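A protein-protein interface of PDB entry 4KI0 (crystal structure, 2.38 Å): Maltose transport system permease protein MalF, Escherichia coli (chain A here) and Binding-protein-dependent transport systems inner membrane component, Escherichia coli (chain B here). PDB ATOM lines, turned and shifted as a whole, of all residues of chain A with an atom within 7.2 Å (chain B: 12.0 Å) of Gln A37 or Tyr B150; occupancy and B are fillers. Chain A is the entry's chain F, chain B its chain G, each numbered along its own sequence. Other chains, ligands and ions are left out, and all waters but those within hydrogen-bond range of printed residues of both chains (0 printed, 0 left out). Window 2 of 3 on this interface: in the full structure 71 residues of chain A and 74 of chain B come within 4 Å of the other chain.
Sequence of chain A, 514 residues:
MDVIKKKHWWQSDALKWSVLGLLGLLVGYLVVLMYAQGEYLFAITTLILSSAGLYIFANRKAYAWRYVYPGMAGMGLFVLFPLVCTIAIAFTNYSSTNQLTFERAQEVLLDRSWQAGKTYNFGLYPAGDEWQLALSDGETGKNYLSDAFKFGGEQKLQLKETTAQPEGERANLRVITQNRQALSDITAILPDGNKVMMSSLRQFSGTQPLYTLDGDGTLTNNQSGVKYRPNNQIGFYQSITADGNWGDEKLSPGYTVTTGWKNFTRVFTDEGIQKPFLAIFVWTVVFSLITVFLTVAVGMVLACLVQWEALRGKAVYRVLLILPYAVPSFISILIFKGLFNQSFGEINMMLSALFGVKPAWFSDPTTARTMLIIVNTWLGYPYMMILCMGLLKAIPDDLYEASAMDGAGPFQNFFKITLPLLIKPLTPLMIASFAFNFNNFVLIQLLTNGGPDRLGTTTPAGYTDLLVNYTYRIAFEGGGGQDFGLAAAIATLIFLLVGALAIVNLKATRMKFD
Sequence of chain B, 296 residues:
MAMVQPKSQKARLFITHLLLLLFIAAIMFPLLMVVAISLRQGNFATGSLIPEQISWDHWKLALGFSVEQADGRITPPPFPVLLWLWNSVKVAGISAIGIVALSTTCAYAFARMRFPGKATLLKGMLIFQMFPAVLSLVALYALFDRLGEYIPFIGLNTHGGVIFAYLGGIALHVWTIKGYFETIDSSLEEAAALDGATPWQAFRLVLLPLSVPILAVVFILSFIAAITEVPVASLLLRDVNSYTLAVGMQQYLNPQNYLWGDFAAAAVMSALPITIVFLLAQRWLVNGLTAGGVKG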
ATOM      1  N   LEU A  30      -8.939   9.416  17.389  1.00  0.00           N
ATOM      2  CA  LEU A  30      -7.544   9.736  17.089  1.00  0.00           C
ATOM      3  C   LEU A  30      -7.042   9.025  15.826  1.00  0.00           C
ATOM      4  O   LEU A  30      -6.188   9.559  15.126  1.00  0.00           O
ATOM      5  CB  LEU A  30      -6.632   9.393  18.275  1.00  0.00           C
ATOM      6  CG  LEU A  30      -6.597  10.364  19.461  1.00  0.00           C
ATOM      7  CD1 LEU A  30      -5.824   9.760  20.625  1.00  0.00           C
ATOM      8  CD2 LEU A  30      -5.987  11.700  19.064  1.00  0.00           C
ATOM      9  N   VAL A  32      -8.949   7.939  13.005  1.00  0.00           N
ATOM     10  CA  VAL A  32      -9.551   8.536  11.805  1.00  0.00           C
ATOM     11  C   VAL A  32      -8.963   9.932  11.586  1.00  0.00           C
ATOM     12  O   VAL A  32      -8.666  10.323  10.458  1.00  0.00           O
ATOM     13  CB  VAL A  32     -11.094   8.607  11.908  1.00  0.00           C
ATOM     14  CG1 VAL A  32     -11.686   9.389  10.741  1.00  0.00           C
ATOM     15  CG2 VAL A  32     -11.698   7.207  11.958  1.00  0.00           C
ATOM     16  N   LEU A  33      -8.775  10.662  12.680  1.00  0.00           N
ATOM     17  CA  LEU A  33      -8.148  11.982  12.650  1.00  0.00           C
ATOM     18  C   LEU A  33      -6.708  11.910  12.113  1.00  0.00           C
ATOM     19  O   LEU A  33      -6.221  12.863  11.508  1.00  0.00           O
ATOM     20  CB  LEU A  33      -8.199  12.598  14.058  1.00  0.00           C
ATOM     21  CG  LEU A  33      -7.912  14.086  14.295  1.00  0.00           C
ATOM     22  CD1 LEU A  33      -6.419  14.376  14.329  1.00  0.00           C
ATOM     23  CD2 LEU A  33      -8.616  14.965  13.268  1.00  0.00           C
ATOM     24  N   MET A  34      -6.037  10.780  12.332  1.00  0.00           N
ATOM     25  CA  MET A  34      -4.723  10.517  11.727  1.00  0.00           C
ATOM     26  C   MET A  34      -4.840  10.077  10.266  1.00  0.00           C
ATOM     27  O   MET A  34      -3.908  10.277   9.485  1.00  0.00           O
ATOM     28  CB  MET A  34      -3.967   9.432  12.504  1.00  0.00           C
ATOM     29  CG  MET A  34      -3.363   9.893  13.815  1.00  0.00           C
ATOM     30  SD  MET A  34      -2.973   8.503  14.893  1.00  0.00           S
ATOM     31  CE  MET A  34      -2.350   9.371  16.329  1.00  0.00           C
ATOM     32  N   TYR A  35      -5.964   9.451   9.912  1.00  0.00           N
ATOM     33  CA  TYR A  35      -6.214   9.024   8.533  1.00  0.00           C
ATOM     34  C   TYR A  35      -6.338  10.232   7.609  1.00  0.00           C
ATOM     35  O   TYR A  35      -5.946  10.168   6.443  1.00  0.00           O
ATOM     36  CB  TYR A  35      -7.475   8.159   8.438  1.00  0.00           C
ATOM     37  CG  TYR A  35      -7.525   7.303   7.191  1.00  0.00           C
ATOM     38  CD1 TYR A  35      -7.022   6.003   7.196  1.00  0.00           C
ATOM     39  CD2 TYR A  35      -8.068   7.792   6.005  1.00  0.00           C
ATOM     40  CE1 TYR A  35      -7.061   5.214   6.060  1.00  0.00           C
ATOM     41  CE2 TYR A  35      -8.112   7.008   4.861  1.00  0.00           C
ATOM     42  CZ  TYR A  35      -7.606   5.721   4.894  1.00  0.00           C
ATOM     43  OH  TYR A  35      -7.647   4.937   3.763  1.00  0.00           O
ATOM     44  N   ALA A  36      -6.887  11.327   8.137  1.00  0.00           N
ATOM     45  CA  ALA A  36      -6.808  12.635   7.483  1.00  0.00           C
ATOM     46  C   ALA A  36      -5.330  13.009   7.295  1.00  0.00           C
ATOM     47  O   ALA A  36      -4.454  12.226   7.649  1.00  0.00           O
ATOM     48  CB  ALA A  36      -7.545  13.683   8.306  1.00  0.00           C
ATOM     49  N   GLN A  37      -5.048  14.195   6.757  1.00  0.00           N
ATOM     50  CA  GLN A  37      -3.706  14.522   6.229  1.00  0.00           C
ATOM     51  C   GLN A  37      -3.083  13.327   5.481  1.00  0.00           C
ATOM     52  O   GLN A  37      -3.091  13.300   4.248  1.00  0.00           O
ATOM     53  CB  GLN A  37      -2.744  15.106   7.295  1.00  0.00           C
ATOM     54  CG  GLN A  37      -2.932  14.667   8.746  1.00  0.00           C
ATOM     55  CD  GLN A  37      -3.916  15.540   9.507  1.00  0.00           C
ATOM     56  OE1 GLN A  37      -3.642  16.711   9.774  1.00  0.00           O
ATOM     57  NE2 GLN A  37      -5.060  14.971   9.871  1.00  0.00           N
ATOM     58  N   GLY A  38      -2.555  12.353   6.221  1.00  0.00           N
ATOM     59  CA  GLY A  38      -2.101  11.089   5.631  1.00  0.00           C
ATOM     60  C   GLY A  38      -1.077  10.312   6.443  1.00  0.00           C
ATOM     61  O   GLY A  38      -0.153   9.729   5.875  1.00  0.00           O
ATOM     62  N   GLU A  39      -1.244  10.289   7.765  1.00  0.00           N
ATOM     63  CA  GLU A  39      -0.325   9.575   8.656  1.00  0.00           C
ATOM     64  C   GLU A  39      -0.806   8.135   8.814  1.00  0.00           C
ATOM     65  O   GLU A  39      -1.369   7.765   9.846  1.00  0.00           O
ATOM     66  CB  GLU A  39      -0.246  10.270  10.021  1.00  0.00           C
ATOM     67  CG  GLU A  39       0.287  11.699   9.982  1.00  0.00           C
ATOM     68  CD  GLU A  39       1.755  11.788   9.595  1.00  0.00           C
ATOM     69  OE1 GLU A  39       2.507  10.816   9.827  1.00  0.00           O
ATOM     70  OE2 GLU A  39       2.161  12.841   9.059  1.00  0.00           O
ATOM     71  N   TYR A  40      -0.572   7.328   7.781  1.00  0.00           N
ATOM     72  CA  TYR A  40      -1.121   5.969   7.709  1.00  0.00           C
ATOM     73  C   TYR A  40      -0.332   4.976   8.562  1.00  0.00           C
ATOM     74  O   TYR A  40      -0.920   4.194   9.312  1.00  0.00           O
ATOM     75  CB  TYR A  40      -1.180   5.496   6.255  1.00  0.00           C
ATOM     76  CG  TYR A  40      -1.974   6.425   5.363  1.00  0.00           C
ATOM     77  CD1 TYR A  40      -1.350   7.169   4.365  1.00  0.00           C
ATOM     78  CD2 TYR A  40      -3.347   6.577   5.535  1.00  0.00           C
ATOM     79  CE1 TYR A  40      -2.074   8.026   3.553  1.00  0.00           C
ATOM     80  CE2 TYR A  40      -4.079   7.432   4.729  1.00  0.00           C
ATOM     81  CZ  TYR A  40      -3.439   8.152   3.740  1.00  0.00           C
ATOM     82  OH  TYR A  40      -4.163   9.001   2.937  1.00  0.00           O
ATOM     83  N   PHE A  42       1.216   5.796  11.069  1.00  0.00           N
ATOM     84  CA  PHE A  42       0.884   6.233  12.425  1.00  0.00           C
ATOM     85  C   PHE A  42      -0.534   5.851  12.853  1.00  0.00           C
ATOM     86  O   PHE A  42      -0.763   5.558  14.019  1.00  0.00           O
ATOM     87  CB  PHE A  42       1.078   7.747  12.562  1.00  0.00           C
ATOM     88  CG  PHE A  42       1.530   8.174  13.928  1.00  0.00           C
ATOM     89  CD1 PHE A  42       0.654   8.794  14.808  1.00  0.00           C
ATOM     90  CD2 PHE A  42       2.838   7.945  14.337  1.00  0.00           C
ATOM     91  CE1 PHE A  42       1.075   9.185  16.069  1.00  0.00           C
ATOM     92  CE2 PHE A  42       3.266   8.332  15.596  1.00  0.00           C
ATOM     93  CZ  PHE A  42       2.382   8.953  16.465  1.00  0.00           C
ATOM     94  N   TYR B 141      12.724  11.992  16.828  1.00  0.00           N
ATOM     95  CA  TYR B 141      12.263  13.315  16.417  1.00  0.00           C
ATOM     96  C   TYR B 141      10.975  13.191  15.622  1.00  0.00           C
ATOM     97  O   TYR B 141      10.006  13.913  15.874  1.00  0.00           O
ATOM     98  CB  TYR B 141      13.304  14.056  15.581  1.00  0.00           C
ATOM     99  CG  TYR B 141      12.953  15.516  15.364  1.00  0.00           C
ATOM    100  CD1 TYR B 141      13.259  16.471  16.324  1.00  0.00           C
ATOM    101  CD2 TYR B 141      12.298  15.933  14.215  1.00  0.00           C
ATOM    102  CE1 TYR B 141      12.932  17.803  16.138  1.00  0.00           C
ATOM    103  CE2 TYR B 141      11.965  17.261  14.019  1.00  0.00           C
ATOM    104  CZ  TYR B 141      12.288  18.195  14.983  1.00  0.00           C
ATOM    105  OH  TYR B 141      11.966  19.521  14.794  1.00  0.00           O
ATOM    106  N   ALA B 142      10.977  12.262  14.671  1.00  0.00           N
ATOM    107  CA  ALA B 142       9.835  12.046  13.792  1.00  0.00           C
ATOM    108  C   ALA B 142       8.606  11.585  14.575  1.00  0.00           C
ATOM    109  O   ALA B 142       7.497  12.042  14.319  1.00  0.00           O
ATOM    110  CB  ALA B 142      10.191  11.034  12.715  1.00  0.00           C
ATOM    111  N   LEU B 143       8.807  10.695  15.541  1.00  0.00           N
ATOM    112  CA  LEU B 143       7.700  10.221  16.367  1.00  0.00           C
ATOM    113  C   LEU B 143       7.089  11.375  17.163  1.00  0.00           C
ATOM    114  O   LEU B 143       5.881  11.598  17.113  1.00  0.00           O
ATOM    115  CB  LEU B 143       8.150   9.082  17.285  1.00  0.00           C
ATOM    116  CG  LEU B 143       7.251   8.697  18.464  1.00  0.00           C
ATOM    117  CD1 LEU B 143       5.861   8.306  18.013  1.00  0.00           C
ATOM    118  CD2 LEU B 143       7.884   7.564  19.251  1.00  0.00           C
ATOM    119  N   PHE B 144       7.927  12.128  17.871  1.00  0.00           N
ATOM    120  CA  PHE B 144       7.424  13.199  18.731  1.00  0.00           C
ATOM    121  C   PHE B 144       6.852  14.380  17.945  1.00  0.00           C
ATOM    122  O   PHE B 144       5.953  15.074  18.428  1.00  0.00           O
ATOM    123  CB  PHE B 144       8.496  13.659  19.713  1.00  0.00           C
ATOM    124  CG  PHE B 144       8.650  12.749  20.892  1.00  0.00           C
ATOM    125  CD1 PHE B 144       9.724  11.876  20.987  1.00  0.00           C
ATOM    126  CD2 PHE B 144       7.702  12.753  21.904  1.00  0.00           C
ATOM    127  CE1 PHE B 144       9.847  11.034  22.071  1.00  0.00           C
ATOM    128  CE2 PHE B 144       7.825  11.913  22.998  1.00  0.00           C
ATOM    129  CZ  PHE B 144       8.897  11.051  23.079  1.00  0.00           C
ATOM    130  N   ASP B 145       7.353  14.592  16.735  1.00  0.00           N
ATOM    131  CA  ASP B 145       6.816  15.635  15.878  1.00  0.00           C
ATOM    132  C   ASP B 145       5.372  15.332  15.477  1.00  0.00           C
ATOM    133  O   ASP B 145       4.521  16.222  15.497  1.00  0.00           O
ATOM    134  CB  ASP B 145       7.687  15.801  14.634  1.00  0.00           C
ATOM    135  CG  ASP B 145       7.410  17.090  13.889  1.00  0.00           C
ATOM    136  OD1 ASP B 145       6.673  17.959  14.408  1.00  0.00           O
ATOM    137  OD2 ASP B 145       7.947  17.236  12.775  1.00  0.00           O
ATOM    138  N   ARG B 146       5.100  14.081  15.113  1.00  0.00           N
ATOM    139  CA  ARG B 146       3.742  13.665  14.761  1.00  0.00           C
ATOM    140  C   ARG B 146       2.861  13.617  16.004  1.00  0.00           C
ATOM    141  O   ARG B 146       1.750  14.149  16.010  1.00  0.00           O
ATOM    142  CB  ARG B 146       3.730  12.288  14.076  1.00  0.00           C
ATOM    143  CG  ARG B 146       3.912  12.311  12.563  1.00  0.00           C
ATOM    144  CD  ARG B 146       5.379  12.312  12.171  1.00  0.00           C
ATOM    145  NE  ARG B 146       5.586  12.317  10.722  1.00  0.00           N
ATOM    146  CZ  ARG B 146       6.768  12.489  10.129  1.00  0.00           C
ATOM    147  NH1 ARG B 146       7.872  12.678  10.854  1.00  0.00           N
ATOM    148  NH2 ARG B 146       6.849  12.481   8.804  1.00  0.00           N
ATOM    149  N   LEU B 147       3.362  12.965  17.045  1.00  0.00           N
ATOM    150  CA  LEU B 147       2.648  12.855  18.314  1.00  0.00           C
ATOM    151  C   LEU B 147       2.158  14.223  18.797  1.00  0.00           C
ATOM    152  O   LEU B 147       1.031  14.347  19.278  1.00  0.00           O
ATOM    153  CB  LEU B 147       3.558  12.205  19.362  1.00  0.00           C
ATOM    154  CG  LEU B 147       2.988  11.725  20.698  1.00  0.00           C
ATOM    155  CD1 LEU B 147       1.796  10.803  20.516  1.00  0.00           C
ATOM    156  CD2 LEU B 147       4.087  11.011  21.464  1.00  0.00           C
ATOM    157  N   GLY B 148       2.997  15.245  18.637  1.00  0.00           N
ATOM    158  CA  GLY B 148       2.667  16.616  19.037  1.00  0.00           C
ATOM    159  C   GLY B 148       1.406  17.200  18.416  1.00  0.00           C
ATOM    160  O   GLY B 148       0.701  17.981  19.048  1.00  0.00           O
ATOM    161  N   GLU B 149       1.129  16.828  17.170  1.00  0.00           N
ATOM    162  CA  GLU B 149      -0.082  17.260  16.479  1.00  0.00           C
ATOM    163  C   GLU B 149      -1.348  16.694  17.146  1.00  0.00           C
ATOM    164  O   GLU B 149      -2.404  17.314  17.092  1.00  0.00           O
ATOM    165  CB  GLU B 149      -0.005  16.842  15.004  1.00  0.00           C
ATOM    166  CG  GLU B 149      -1.181  17.267  14.122  1.00  0.00           C
ATOM    167  CD  GLU B 149      -1.309  18.771  13.943  1.00  0.00           C
ATOM    168  OE1 GLU B 149      -0.307  19.499  14.125  1.00  0.00           O
ATOM    169  OE2 GLU B 149      -2.425  19.224  13.605  1.00  0.00           O
ATOM    170  N   TYR B 150      -1.235  15.535  17.795  1.00  0.00           N
ATOM    171  CA  TYR B 150      -2.395  14.859  18.379  1.00  0.00           C
ATOM    172  C   TYR B 150      -2.465  14.973  19.914  1.00  0.00           C
ATOM    173  O   TYR B 150      -3.503  15.355  20.445  1.00  0.00           O
ATOM    174  CB  TYR B 150      -2.429  13.402  17.901  1.00  0.00           C
ATOM    175  CG  TYR B 150      -2.285  13.302  16.392  1.00  0.00           C
ATOM    176  CD1 TYR B 150      -1.113  12.826  15.809  1.00  0.00           C
ATOM    177  CD2 TYR B 150      -3.301  13.730  15.548  1.00  0.00           C
ATOM    178  CE1 TYR B 150      -0.972  12.755  14.429  1.00  0.00           C
ATOM    179  CE2 TYR B 150      -3.168  13.664  14.167  1.00  0.00           C
ATOM    180  CZ  TYR B 150      -2.002  13.176  13.612  1.00  0.00           C
ATOM    181  OH  TYR B 150      -1.876  13.109  12.239  1.00  0.00           O
ATOM    182  N   ILE B 151      -1.384  14.644  20.623  1.00  0.00           N
ATOM    183  CA  ILE B 151      -1.291  14.922  22.068  1.00  0.00           C
ATOM    184  C   ILE B 151      -0.134  15.897  22.315  1.00  0.00           C
ATOM    185  O   ILE B 151       0.995  15.475  22.549  1.00  0.00           O
ATOM    186  CB  ILE B 151      -1.094  13.646  22.925  1.00  0.00           C
ATOM    187  CG1 ILE B 151      -2.067  12.538  22.504  1.00  0.00           C
ATOM    188  CG2 ILE B 151      -1.280  13.963  24.407  1.00  0.00           C
ATOM    189  CD1 ILE B 151      -1.479  11.526  21.543  1.00  0.00           C
ATOM    190  N   PRO B 152      -0.410  17.214  22.258  1.00  0.00           N
ATOM    191  CA  PRO B 152       0.671  18.209  22.363  1.00  0.00           C
ATOM    192  C   PRO B 152       1.379  18.229  23.718  1.00  0.00           C
ATOM    193  O   PRO B 152       2.517  18.671  23.801  1.00  0.00           O
ATOM    194  CB  PRO B 152      -0.036  19.545  22.098  1.00  0.00           C
ATOM    195  CG  PRO B 152      -1.483  19.298  22.346  1.00  0.00           C
ATOM    196  CD  PRO B 152      -1.734  17.843  22.078  1.00  0.00           C
ATOM    197  N   PHE B 153       0.703  17.738  24.752  1.00  0.00           N
ATOM    198  CA  PHE B 153       1.250  17.632  26.103  1.00  0.00           C
ATOM    199  C   PHE B 153       2.478  16.711  26.180  1.00  0.00           C
ATOM    200  O   PHE B 153       3.268  16.804  27.116  1.00  0.00           O
ATOM    201  CB  PHE B 153       0.138  17.131  27.042  1.00  0.00           C
ATOM    202  CG  PHE B 153       0.500  17.146  28.504  1.00  0.00           C
ATOM    203  CD1 PHE B 153       0.941  18.317  29.120  1.00  0.00           C
ATOM    204  CD2 PHE B 153       0.365  15.994  29.279  1.00  0.00           C
ATOM    205  CE1 PHE B 153       1.265  18.333  30.469  1.00  0.00           C
ATOM    206  CE2 PHE B 153       0.685  16.004  30.630  1.00  0.00           C
ATOM    207  CZ  PHE B 153       1.133  17.177  31.224  1.00  0.00           C
ATOM    208  N   ILE B 154       2.643  15.828  25.198  1.00  0.00           N
ATOM    209  CA  ILE B 154       3.810  14.944  25.149  1.00  0.00           C
ATOM    210  C   ILE B 154       4.562  14.998  23.810  1.00  0.00           C
ATOM    211  O   ILE B 154       5.221  14.035  23.439  1.00  0.00           O
ATOM    212  CB  ILE B 154       3.426  13.483  25.496  1.00  0.00           C
ATOM    213  CG1 ILE B 154       2.369  12.937  24.525  1.00  0.00           C
ATOM    214  CG2 ILE B 154       2.919  13.398  26.929  1.00  0.00           C
ATOM    215  CD1 ILE B 154       1.970  11.506  24.810  1.00  0.00           C
ATOM    216  N   GLY B 155       4.477  16.130  23.106  1.00  0.00           N
ATOM    217  CA  GLY B 155       5.193  16.332  21.836  1.00  0.00           C
ATOM    218  C   GLY B 155       6.535  17.031  22.013  1.00  0.00           C
ATOM    219  O   GLY B 155       7.043  17.143  23.120  1.00  0.00           O
ATOM    220  N   LEU B 156       7.110  17.507  20.912  1.00  0.00           N
ATOM    221  CA  LEU B 156       8.366  18.256  20.958  1.00  0.00           C
ATOM    222  C   LEU B 156       8.283  19.452  21.897  1.00  0.00           C
ATOM    223  O   LEU B 156       7.213  20.039  22.082  1.00  0.00           O
ATOM    224  CB  LEU B 156       8.744  18.771  19.567  1.00  0.00           C
ATOM    225  CG  LEU B 156       9.169  17.751  18.513  1.00  0.00           C
ATOM    226  CD1 LEU B 156       9.421  18.464  17.195  1.00  0.00           C
ATOM    227  CD2 LEU B 156      10.406  16.989  18.960  1.00  0.00           C
ATOM    228  N   THR B 158       8.489  19.663  25.163  1.00  0.00           N
ATOM    229  CA  THR B 158       7.705  19.440  26.371  1.00  0.00           C
ATOM    230  C   THR B 158       8.430  18.474  27.272  1.00  0.00           C
ATOM    231  O   THR B 158       9.141  17.592  26.792  1.00  0.00           O
ATOM    232  CB  THR B 158       6.359  18.774  26.074  1.00  0.00           C
ATOM    233  OG1 THR B 158       6.588  17.435  25.617  1.00  0.00           O
ATOM    234  CG2 THR B 158       5.560  19.562  25.037  1.00  0.00           C
ATOM    235  N   GLY B 161       7.152  14.835  26.875  1.00  0.00           N
ATOM    236  CA  GLY B 161       7.826  14.111  25.803  1.00  0.00           C
ATOM    237  C   GLY B 161       9.127  13.481  26.242  1.00  0.00           C
ATOM    238  O   GLY B 161       9.372  12.313  25.994  1.00  0.00           O
ATOM    239  N   PHE B 164       8.252  10.688  28.571  1.00  0.00           N
ATOM    240  CA  PHE B 164       7.647   9.601  27.843  1.00  0.00           C
ATOM    241  C   PHE B 164       8.731   8.795  27.135  1.00  0.00           C
ATOM    242  O   PHE B 164       8.671   7.574  27.108  1.00  0.00           O
ATOM    243  CB  PHE B 164       6.601  10.158  26.864  1.00  0.00           C
ATOM    244  CG  PHE B 164       5.667   9.128  26.293  1.00  0.00           C
ATOM    245  CD1 PHE B 164       5.210   8.057  27.055  1.00  0.00           C
ATOM    246  CD2 PHE B 164       5.208   9.254  24.982  1.00  0.00           C
ATOM    247  CE1 PHE B 164       4.348   7.121  26.510  1.00  0.00           C
ATOM    248  CE2 PHE B 164       4.340   8.321  24.438  1.00  0.00           C
ATOM    249  CZ  PHE B 164       3.909   7.253  25.203  1.00  0.00           C
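The side-chain carboxylate (OE1) of Glu A39 is in salt-bridge range of the guanidinium group (NE) of Arg B146 (3.5 Å).
O of Leu A33 is in hydrogen-bond range of NE2 of Gln A37 (2.9 Å).
The backbone NH (N) of Glu A39 lies within hydrogen-bond range of the backbone carbonyl oxygen (O) of Met A34 (3.2 Å).
CE2 of Tyr B150 touches CD1 of Leu A33 (3.3 Å).
CG of Met A34 touches CZ of Tyr B150, 3.6 Å away.
Tyr B150 touches Gln A37 (OH to CG, 3.97 Å).
Tyr B150 touches Glu A39 (OH to CG, 3.4 Å).
Leu B143 touches Phe A42.
Gln A37 touches one residue of chain B.
Of chain A, only Leu A33 (3.3 Å), Met A34 (3.6 Å), Gln A37 (3.97 Å) and Glu A39 (3.4 Å) come within 4 Å of Tyr B150.
No residue of chain B comes within 4 Å of Leu A30.
Leu A33 touches just one residue of chain B: Tyr B150.
No residue of chain B comes within 4 Å of Ala A36.
Gly A38 touches none of the printed residues of chain B.
Printed residues of chain B within 4 Å of Phe A42: Leu B143.
Of the printed residues of chain A, Leu B143 touches Phe A42.
Of the printed residues of chain A, Arg B146 touches Glu A39 (3.4 Å).
Leu B147 touches none of the printed residues of chain A.
Tyr A35 touches none of the printed residues of chain B.
The nearest printed residue of chain B that does not touch Phe A42 is Leu B147 (4.2 Å).
Of the 19 printed residues of chain B, 3 touch a printed residue of chain A.
Printed residues of chain B that touch a printed residue of chain A: Leu B143, Arg B146 and Tyr B150.
Hydrophobic or aromatic side chains of chain B within 4 Å of the printed part of chain A: Leu B143 and Tyr B150.
Of the 11 printed residues of chain A, 5 touch a printed residue of chain B.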
